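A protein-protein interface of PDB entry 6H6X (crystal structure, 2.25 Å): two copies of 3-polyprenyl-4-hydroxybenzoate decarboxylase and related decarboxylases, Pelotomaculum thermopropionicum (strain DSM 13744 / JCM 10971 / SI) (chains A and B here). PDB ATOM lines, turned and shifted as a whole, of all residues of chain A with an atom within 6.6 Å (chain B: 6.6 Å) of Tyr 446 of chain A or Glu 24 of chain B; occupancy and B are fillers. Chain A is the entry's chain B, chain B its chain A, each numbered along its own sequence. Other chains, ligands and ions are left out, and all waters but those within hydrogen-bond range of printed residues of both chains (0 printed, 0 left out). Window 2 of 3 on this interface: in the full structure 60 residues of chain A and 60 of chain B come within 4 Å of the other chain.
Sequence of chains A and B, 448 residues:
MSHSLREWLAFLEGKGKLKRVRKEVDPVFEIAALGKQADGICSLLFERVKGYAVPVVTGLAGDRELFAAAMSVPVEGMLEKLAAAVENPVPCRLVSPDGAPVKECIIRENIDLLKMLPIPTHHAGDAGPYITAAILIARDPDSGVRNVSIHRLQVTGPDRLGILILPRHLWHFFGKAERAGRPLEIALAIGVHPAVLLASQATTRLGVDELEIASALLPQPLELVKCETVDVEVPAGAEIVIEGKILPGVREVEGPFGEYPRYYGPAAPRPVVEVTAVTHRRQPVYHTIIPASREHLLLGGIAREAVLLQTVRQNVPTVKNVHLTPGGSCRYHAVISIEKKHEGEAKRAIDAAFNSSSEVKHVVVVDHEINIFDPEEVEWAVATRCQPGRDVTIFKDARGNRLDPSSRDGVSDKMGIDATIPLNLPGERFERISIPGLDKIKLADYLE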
ATOM      1  N   ILE A 441     -25.563  -4.819 -33.110  1.00  0.00           N
ATOM      2  CA  ILE A 441     -25.785  -3.702 -32.157  1.00  0.00           C
ATOM      3  C   ILE A 441     -24.611  -2.708 -32.192  1.00  0.00           C
ATOM      4  O   ILE A 441     -23.459  -3.113 -32.138  1.00  0.00           O
ATOM      5  CB  ILE A 441     -26.019  -4.221 -30.716  1.00  0.00           C
ATOM      6  CG1 ILE A 441     -27.227  -5.185 -30.652  1.00  0.00           C
ATOM      7  CG2 ILE A 441     -26.223  -3.061 -29.747  1.00  0.00           C
ATOM      8  CD1 ILE A 441     -28.573  -4.630 -31.123  1.00  0.00           C
ATOM      9  N   LYS A 442     -24.917  -1.415 -32.286  1.00  0.00           N
ATOM     10  CA  LYS A 442     -23.932  -0.377 -32.546  1.00  0.00           C
ATOM     11  C   LYS A 442     -23.932   0.663 -31.433  1.00  0.00           C
ATOM     12  O   LYS A 442     -24.978   1.187 -31.067  1.00  0.00           O
ATOM     13  CB  LYS A 442     -24.209   0.319 -33.895  1.00  0.00           C
ATOM     14  CG  LYS A 442     -23.909  -0.518 -35.127  1.00  0.00           C
ATOM     15  CD  LYS A 442     -22.421  -0.499 -35.468  1.00  0.00           C
ATOM     16  CE  LYS A 442     -21.999  -1.683 -36.345  1.00  0.00           C
ATOM     17  NZ  LYS A 442     -20.524  -1.759 -36.543  1.00  0.00           N
ATOM     18  N   LEU A 443     -22.743   0.987 -30.943  1.00  0.00           N
ATOM     19  CA  LEU A 443     -22.588   1.890 -29.818  1.00  0.00           C
ATOM     20  C   LEU A 443     -23.110   3.278 -30.139  1.00  0.00           C
ATOM     21  O   LEU A 443     -23.760   3.904 -29.288  1.00  0.00           O
ATOM     22  CB  LEU A 443     -21.127   1.994 -29.374  1.00  0.00           C
ATOM     23  CG  LEU A 443     -20.855   2.818 -28.105  1.00  0.00           C
ATOM     24  CD1 LEU A 443     -21.682   2.278 -26.940  1.00  0.00           C
ATOM     25  CD2 LEU A 443     -19.378   2.920 -27.754  1.00  0.00           C
ATOM     26  N   ALA A 444     -22.844   3.749 -31.359  1.00  0.00           N
ATOM     27  CA  ALA A 444     -23.319   5.078 -31.816  1.00  0.00           C
ATOM     28  C   ALA A 444     -24.849   5.222 -31.737  1.00  0.00           C
ATOM     29  O   ALA A 444     -25.325   6.267 -31.307  1.00  0.00           O
ATOM     30  CB  ALA A 444     -22.813   5.390 -33.210  1.00  0.00           C
ATOM     31  N   ASP A 445     -25.605   4.166 -32.074  1.00  0.00           N
ATOM     32  CA  ASP A 445     -27.092   4.189 -31.973  1.00  0.00           C
ATOM     33  C   ASP A 445     -27.682   4.185 -30.560  1.00  0.00           C
ATOM     34  O   ASP A 445     -28.905   4.361 -30.422  1.00  0.00           O
ATOM     35  CB  ASP A 445     -27.734   3.008 -32.722  1.00  0.00           C
ATOM     36  CG  ASP A 445     -27.338   2.952 -34.197  1.00  0.00           C
ATOM     37  OD1 ASP A 445     -26.923   3.987 -34.776  1.00  0.00           O
ATOM     38  OD2 ASP A 445     -27.433   1.847 -34.775  1.00  0.00           O
ATOM     39  N   TYR A 446     -26.857   3.945 -29.532  1.00  0.00           N
ATOM     40  CA  TYR A 446     -27.321   3.936 -28.132  1.00  0.00           C
ATOM     41  C   TYR A 446     -26.924   5.161 -27.314  1.00  0.00           C
ATOM     42  O   TYR A 446     -27.562   5.434 -26.305  1.00  0.00           O
ATOM     43  CB  TYR A 446     -26.834   2.671 -27.445  1.00  0.00           C
ATOM     44  CG  TYR A 446     -27.673   1.490 -27.769  1.00  0.00           C
ATOM     45  CD1 TYR A 446     -27.577   0.878 -29.004  1.00  0.00           C
ATOM     46  CD2 TYR A 446     -28.554   0.953 -26.832  1.00  0.00           C
ATOM     47  CE1 TYR A 446     -28.349  -0.222 -29.323  1.00  0.00           C
ATOM     48  CE2 TYR A 446     -29.323  -0.168 -27.121  1.00  0.00           C
ATOM     49  CZ  TYR A 446     -29.228  -0.743 -28.388  1.00  0.00           C
ATOM     50  OH  TYR A 446     -29.918  -1.884 -28.740  1.00  0.00           O
ATOM     51  N   LEU A 447     -25.836   5.824 -27.705  1.00  0.00           N
ATOM     52  CA  LEU A 447     -25.382   7.051 -27.105  1.00  0.00           C
ATOM     53  C   LEU A 447     -25.509   8.115 -28.176  1.00  0.00           C
ATOM     54  O   LEU A 447     -25.688   9.297 -27.890  1.00  0.00           O
ATOM     55  CB  LEU A 447     -23.933   6.918 -26.604  1.00  0.00           C
ATOM     56  CG  LEU A 447     -22.815   6.765 -27.630  1.00  0.00           C
ATOM     57  CD1 LEU A 447     -22.288   8.091 -28.166  1.00  0.00           C
ATOM     58  CD2 LEU A 447     -21.685   6.046 -26.933  1.00  0.00           C
ATOM     59  N   ARG B  20     -22.975   8.321 -21.123  1.00  0.00           N
ATOM     60  CA  ARG B  20     -24.162   7.700 -20.618  1.00  0.00           C
ATOM     61  C   ARG B  20     -24.935   7.096 -21.761  1.00  0.00           C
ATOM     62  O   ARG B  20     -24.872   7.570 -22.895  1.00  0.00           O
ATOM     63  CB  ARG B  20     -24.990   8.766 -19.899  1.00  0.00           C
ATOM     64  CG  ARG B  20     -24.174   9.483 -18.816  1.00  0.00           C
ATOM     65  CD  ARG B  20     -24.901  10.720 -18.347  1.00  0.00           C
ATOM     66  NE  ARG B  20     -24.286  11.237 -17.123  1.00  0.00           N
ATOM     67  CZ  ARG B  20     -24.670  10.920 -15.888  1.00  0.00           C
ATOM     68  NH1 ARG B  20     -25.687  10.074 -15.643  1.00  0.00           N
ATOM     69  NH2 ARG B  20     -24.009  11.447 -14.881  1.00  0.00           N
ATOM     70  N   VAL B  21     -25.679   6.051 -21.447  1.00  0.00           N
ATOM     71  CA  VAL B  21     -26.528   5.392 -22.381  1.00  0.00           C
ATOM     72  C   VAL B  21     -27.924   5.391 -21.770  1.00  0.00           C
ATOM     73  O   VAL B  21     -28.264   4.521 -20.892  1.00  0.00           O
ATOM     74  CB  VAL B  21     -26.041   3.958 -22.627  1.00  0.00           C
ATOM     75  CG1 VAL B  21     -27.014   3.202 -23.513  1.00  0.00           C
ATOM     76  CG2 VAL B  21     -24.642   3.973 -23.235  1.00  0.00           C
ATOM     77  N   ARG B  22     -28.739   6.329 -22.281  1.00  0.00           N
ATOM     78  CA  ARG B  22     -30.112   6.558 -21.812  1.00  0.00           C
ATOM     79  C   ARG B  22     -31.110   5.574 -22.389  1.00  0.00           C
ATOM     80  O   ARG B  22     -32.160   5.365 -21.790  1.00  0.00           O
ATOM     81  CB  ARG B  22     -30.564   7.969 -22.179  1.00  0.00           C
ATOM     82  CG  ARG B  22     -29.670   9.116 -21.757  1.00  0.00           C
ATOM     83  CD  ARG B  22     -30.281  10.429 -22.275  1.00  0.00           C
ATOM     84  NE  ARG B  22     -29.891  11.632 -21.511  1.00  0.00           N
ATOM     85  CZ  ARG B  22     -29.954  12.904 -21.957  1.00  0.00           C
ATOM     86  NH1 ARG B  22     -29.581  13.927 -21.175  1.00  0.00           N
ATOM     87  NH2 ARG B  22     -30.383  13.183 -23.187  1.00  0.00           N
ATOM     88  N   LYS B  23     -30.815   4.985 -23.557  1.00  0.00           N
ATOM     89  CA  LYS B  23     -31.697   3.957 -24.136  1.00  0.00           C
ATOM     90  C   LYS B  23     -31.594   2.679 -23.344  1.00  0.00           C
ATOM     91  O   LYS B  23     -30.513   2.319 -22.891  1.00  0.00           O
ATOM     92  CB  LYS B  23     -31.388   3.677 -25.622  1.00  0.00           C
ATOM     93  CG  LYS B  23     -32.322   4.398 -26.582  1.00  0.00           C
ATOM     94  CD  LYS B  23     -31.914   4.194 -28.032  1.00  0.00           C
ATOM     95  CE  LYS B  23     -32.994   4.692 -28.990  1.00  0.00           C
ATOM     96  NZ  LYS B  23     -32.478   4.942 -30.367  1.00  0.00           N
ATOM     97  N   GLU B  24     -32.722   1.997 -23.209  1.00  0.00           N
ATOM     98  CA  GLU B  24     -32.823   0.775 -22.448  1.00  0.00           C
ATOM     99  C   GLU B  24     -31.923  -0.304 -23.069  1.00  0.00           C
ATOM    100  O   GLU B  24     -31.864  -0.434 -24.291  1.00  0.00           O
ATOM    101  CB  GLU B  24     -34.278   0.297 -22.354  1.00  0.00           C
ATOM    102  CG  GLU B  24     -34.411  -1.207 -22.140  1.00  0.00           C
ATOM    103  CD  GLU B  24     -35.839  -1.680 -21.953  1.00  0.00           C
ATOM    104  OE1 GLU B  24     -36.253  -2.599 -22.681  1.00  0.00           O
ATOM    105  OE2 GLU B  24     -36.534  -1.172 -21.057  1.00  0.00           O
ATOM    106  N   VAL B  25     -31.231  -1.069 -22.214  1.00  0.00           N
ATOM    107  CA  VAL B  25     -30.372  -2.195 -22.650  1.00  0.00           C
ATOM    108  C   VAL B  25     -30.746  -3.439 -21.879  1.00  0.00           C
ATOM    109  O   VAL B  25     -31.174  -3.365 -20.737  1.00  0.00           O
ATOM    110  CB  VAL B  25     -28.884  -1.876 -22.454  1.00  0.00           C
ATOM    111  CG1 VAL B  25     -28.490  -0.647 -23.245  1.00  0.00           C
ATOM    112  CG2 VAL B  25     -28.558  -1.607 -20.989  1.00  0.00           C
ATOM    113  N   ASP B  26     -30.592  -4.598 -22.485  1.00  0.00           N
ATOM    114  CA  ASP B  26     -30.803  -5.865 -21.772  1.00  0.00           C
ATOM    115  C   ASP B  26     -29.489  -6.233 -21.006  1.00  0.00           C
ATOM    116  O   ASP B  26     -28.402  -6.223 -21.591  1.00  0.00           O
ATOM    117  CB  ASP B  26     -31.147  -6.959 -22.804  1.00  0.00           C
ATOM    118  CG  ASP B  26     -31.797  -8.216 -22.197  1.00  0.00           C
ATOM    119  OD1 ASP B  26     -31.572  -8.589 -21.031  1.00  0.00           O
ATOM    120  OD2 ASP B  26     -32.550  -8.880 -22.934  1.00  0.00           O
ATOM    121  N   GLU B  30     -26.358  -7.643 -24.013  1.00  0.00           N
ATOM    122  CA  GLU B  30     -26.230  -6.333 -24.628  1.00  0.00           C
ATOM    123  C   GLU B  30     -25.272  -5.413 -23.909  1.00  0.00           C
ATOM    124  O   GLU B  30     -24.593  -4.601 -24.567  1.00  0.00           O
ATOM    125  CB  GLU B  30     -27.586  -5.639 -24.787  1.00  0.00           C
ATOM    126  CG  GLU B  30     -28.506  -6.314 -25.792  1.00  0.00           C
ATOM    127  CD  GLU B  30     -29.704  -5.444 -26.180  1.00  0.00           C
ATOM    128  OE1 GLU B  30     -30.106  -4.552 -25.387  1.00  0.00           O
ATOM    129  OE2 GLU B  30     -30.220  -5.652 -27.313  1.00  0.00           O
ATOM    130  N   LEU B  34     -22.204  -3.778 -25.947  1.00  0.00           N
ATOM    131  CA  LEU B  34     -21.929  -2.349 -26.061  1.00  0.00           C
ATOM    132  C   LEU B  34     -20.659  -1.992 -25.347  1.00  0.00           C
ATOM    133  O   LEU B  34     -19.865  -1.162 -25.820  1.00  0.00           O
ATOM    134  CB  LEU B  34     -23.108  -1.583 -25.495  1.00  0.00           C
ATOM    135  CG  LEU B  34     -24.350  -1.753 -26.372  1.00  0.00           C
ATOM    136  CD1 LEU B  34     -25.654  -1.546 -25.601  1.00  0.00           C
ATOM    137  CD2 LEU B  34     -24.189  -0.766 -27.518  1.00  0.00           C
ATOM    138  N   PHE B  46     -24.917   2.767 -18.008  1.00  0.00           N
ATOM    139  CA  PHE B  46     -26.193   2.365 -18.538  1.00  0.00           C
ATOM    140  C   PHE B  46     -27.353   2.780 -17.621  1.00  0.00           C
ATOM    141  O   PHE B  46     -27.671   2.053 -16.637  1.00  0.00           O
ATOM    142  CB  PHE B  46     -26.229   0.858 -18.766  1.00  0.00           C
ATOM    143  CG  PHE B  46     -25.225   0.379 -19.799  1.00  0.00           C
ATOM    144  CD1 PHE B  46     -25.533   0.389 -21.158  1.00  0.00           C
ATOM    145  CD2 PHE B  46     -23.978  -0.114 -19.410  1.00  0.00           C
ATOM    146  CE1 PHE B  46     -24.618  -0.065 -22.107  1.00  0.00           C
ATOM    147  CE2 PHE B  46     -23.068  -0.576 -20.351  1.00  0.00           C
ATOM    148  CZ  PHE B  46     -23.386  -0.561 -21.701  1.00  0.00           C
ATOM    149  N   ARG B  48     -30.600   2.897 -18.031  1.00  0.00           N
ATOM    150  CA  ARG B  48     -31.825   2.107 -18.046  1.00  0.00           C
ATOM    151  C   ARG B  48     -31.524   0.685 -18.434  1.00  0.00           C
ATOM    152  O   ARG B  48     -31.220   0.399 -19.598  1.00  0.00           O
ATOM    153  CB  ARG B  48     -32.849   2.713 -19.023  1.00  0.00           C
ATOM    154  N   VAL B  49     -31.626  -0.208 -17.462  1.00  0.00           N
ATOM    155  CA  VAL B  49     -31.384  -1.605 -17.668  1.00  0.00           C
ATOM    156  C   VAL B  49     -32.699  -2.316 -17.475  1.00  0.00           C
ATOM    157  O   VAL B  49     -33.348  -2.179 -16.449  1.00  0.00           O
ATOM    158  CB  VAL B  49     -30.292  -2.146 -16.706  1.00  0.00           C
ATOM    159  CG1 VAL B  49     -30.127  -3.644 -16.862  1.00  0.00           C
ATOM    160  CG2 VAL B  49     -28.975  -1.413 -16.959  1.00  0.00           C
ATOM    161  N   LYS B  50     -33.068  -3.091 -18.481  1.00  0.00           N
ATOM    162  CA  LYS B  50     -34.378  -3.691 -18.546  1.00  0.00           C
ATOM    163  C   LYS B  50     -34.605  -4.516 -17.289  1.00  0.00           C
ATOM    164  O   LYS B  50     -33.880  -5.482 -17.033  1.00  0.00           O
ATOM    165  CB  LYS B  50     -34.501  -4.561 -19.795  1.00  0.00           C
ATOM    166  CG  LYS B  50     -35.905  -5.132 -20.010  1.00  0.00           C
ATOM    167  CD  LYS B  50     -36.103  -5.764 -21.387  1.00  0.00           C
ATOM    168  CE  LYS B  50     -35.459  -7.140 -21.545  1.00  0.00           C
ATOM    169  NZ  LYS B  50     -36.006  -8.166 -20.614  1.00  0.00           N
ATOM    170  N   GLY B  51     -35.612  -4.105 -16.520  1.00  0.00           N
ATOM    171  CA  GLY B  51     -36.052  -4.837 -15.333  1.00  0.00           C
ATOM    172  C   GLY B  51     -35.602  -4.235 -14.012  1.00  0.00           C
ATOM    173  O   GLY B  51     -35.873  -4.827 -12.961  1.00  0.00           O
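Ile 441 of chain A touches Leu 34 of chain B (CG2 to CD2, 3.8 Å).
Leu 443 of chain A touches Leu 34 of chain B.
O of Asp 445 of chain A touches NZ of Lys 23 of chain B, 3.6 Å away.
Val 21 of chain B touches Tyr 446 of chain A (CG1 to O, 3.6 Å).
Tyr 446 of chain A touches Glu 24 of chain B.
Val 25 of chain B touches Tyr 446 of chain A.
Arg 20 of chain B touches Leu 447 of chain A (O to CB, 3.9 Å).
Hydrophobic or aromatic side chains of chain B that line the printed part of chain A: Val 21, Val 25 and Leu 34.
Of the 7 printed residues of chain A, 5 touch a printed residue of chain B.
Hydrophobic or aromatic side chains of chain A within 4 Å of the printed part of chain B: Ile 441, Leu 443, Tyr 446 and Leu 447.
Among the printed residues, no Asp or Glu carboxylate lies within 4 Å of a Lys or Arg side-chain nitrogen of the other chain.
Of the printed residues of chain B, Leu 443 of chain A touches Leu 34.
Tyr 446 of chain A touches just these residues of chain B: Val 21, Glu 24 and Val 25.
Printed residues of chain A within 4 Å of Val 21 of chain B: Tyr 446.
Glu 24 of chain B touches one residue of chain A.
Of the printed residues of chain A, Val 25 of chain B touches Tyr 446.
Of the printed residues of chain A, Leu 34 of chain B touches Ile 441 (3.8 Å) and Leu 443 (3.9 Å).
The nearest printed residue of chain B that does not touch Tyr 446 of chain A is Leu 34 of chain B (4.02 Å).
The nearest printed residue of chain A that does not touch Glu 24 of chain B is Ile 441 of chain A (8.3 Å).
The nearest printed residue of chain A that does not touch Val 21 of chain B is Leu 447 of chain A (4.5 Å).
No position is printed for both chains.
The backbone NH of Lys 50 of chain B lies within hydrogen-bond range of the backbone carbonyl oxygen of Val 25 of chain B (3.0 Å).
The backbone NH of Val 25 of chain B is in hydrogen-bond range of the backbone carbonyl oxygen of Arg 48 of chain B (3.0 Å).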
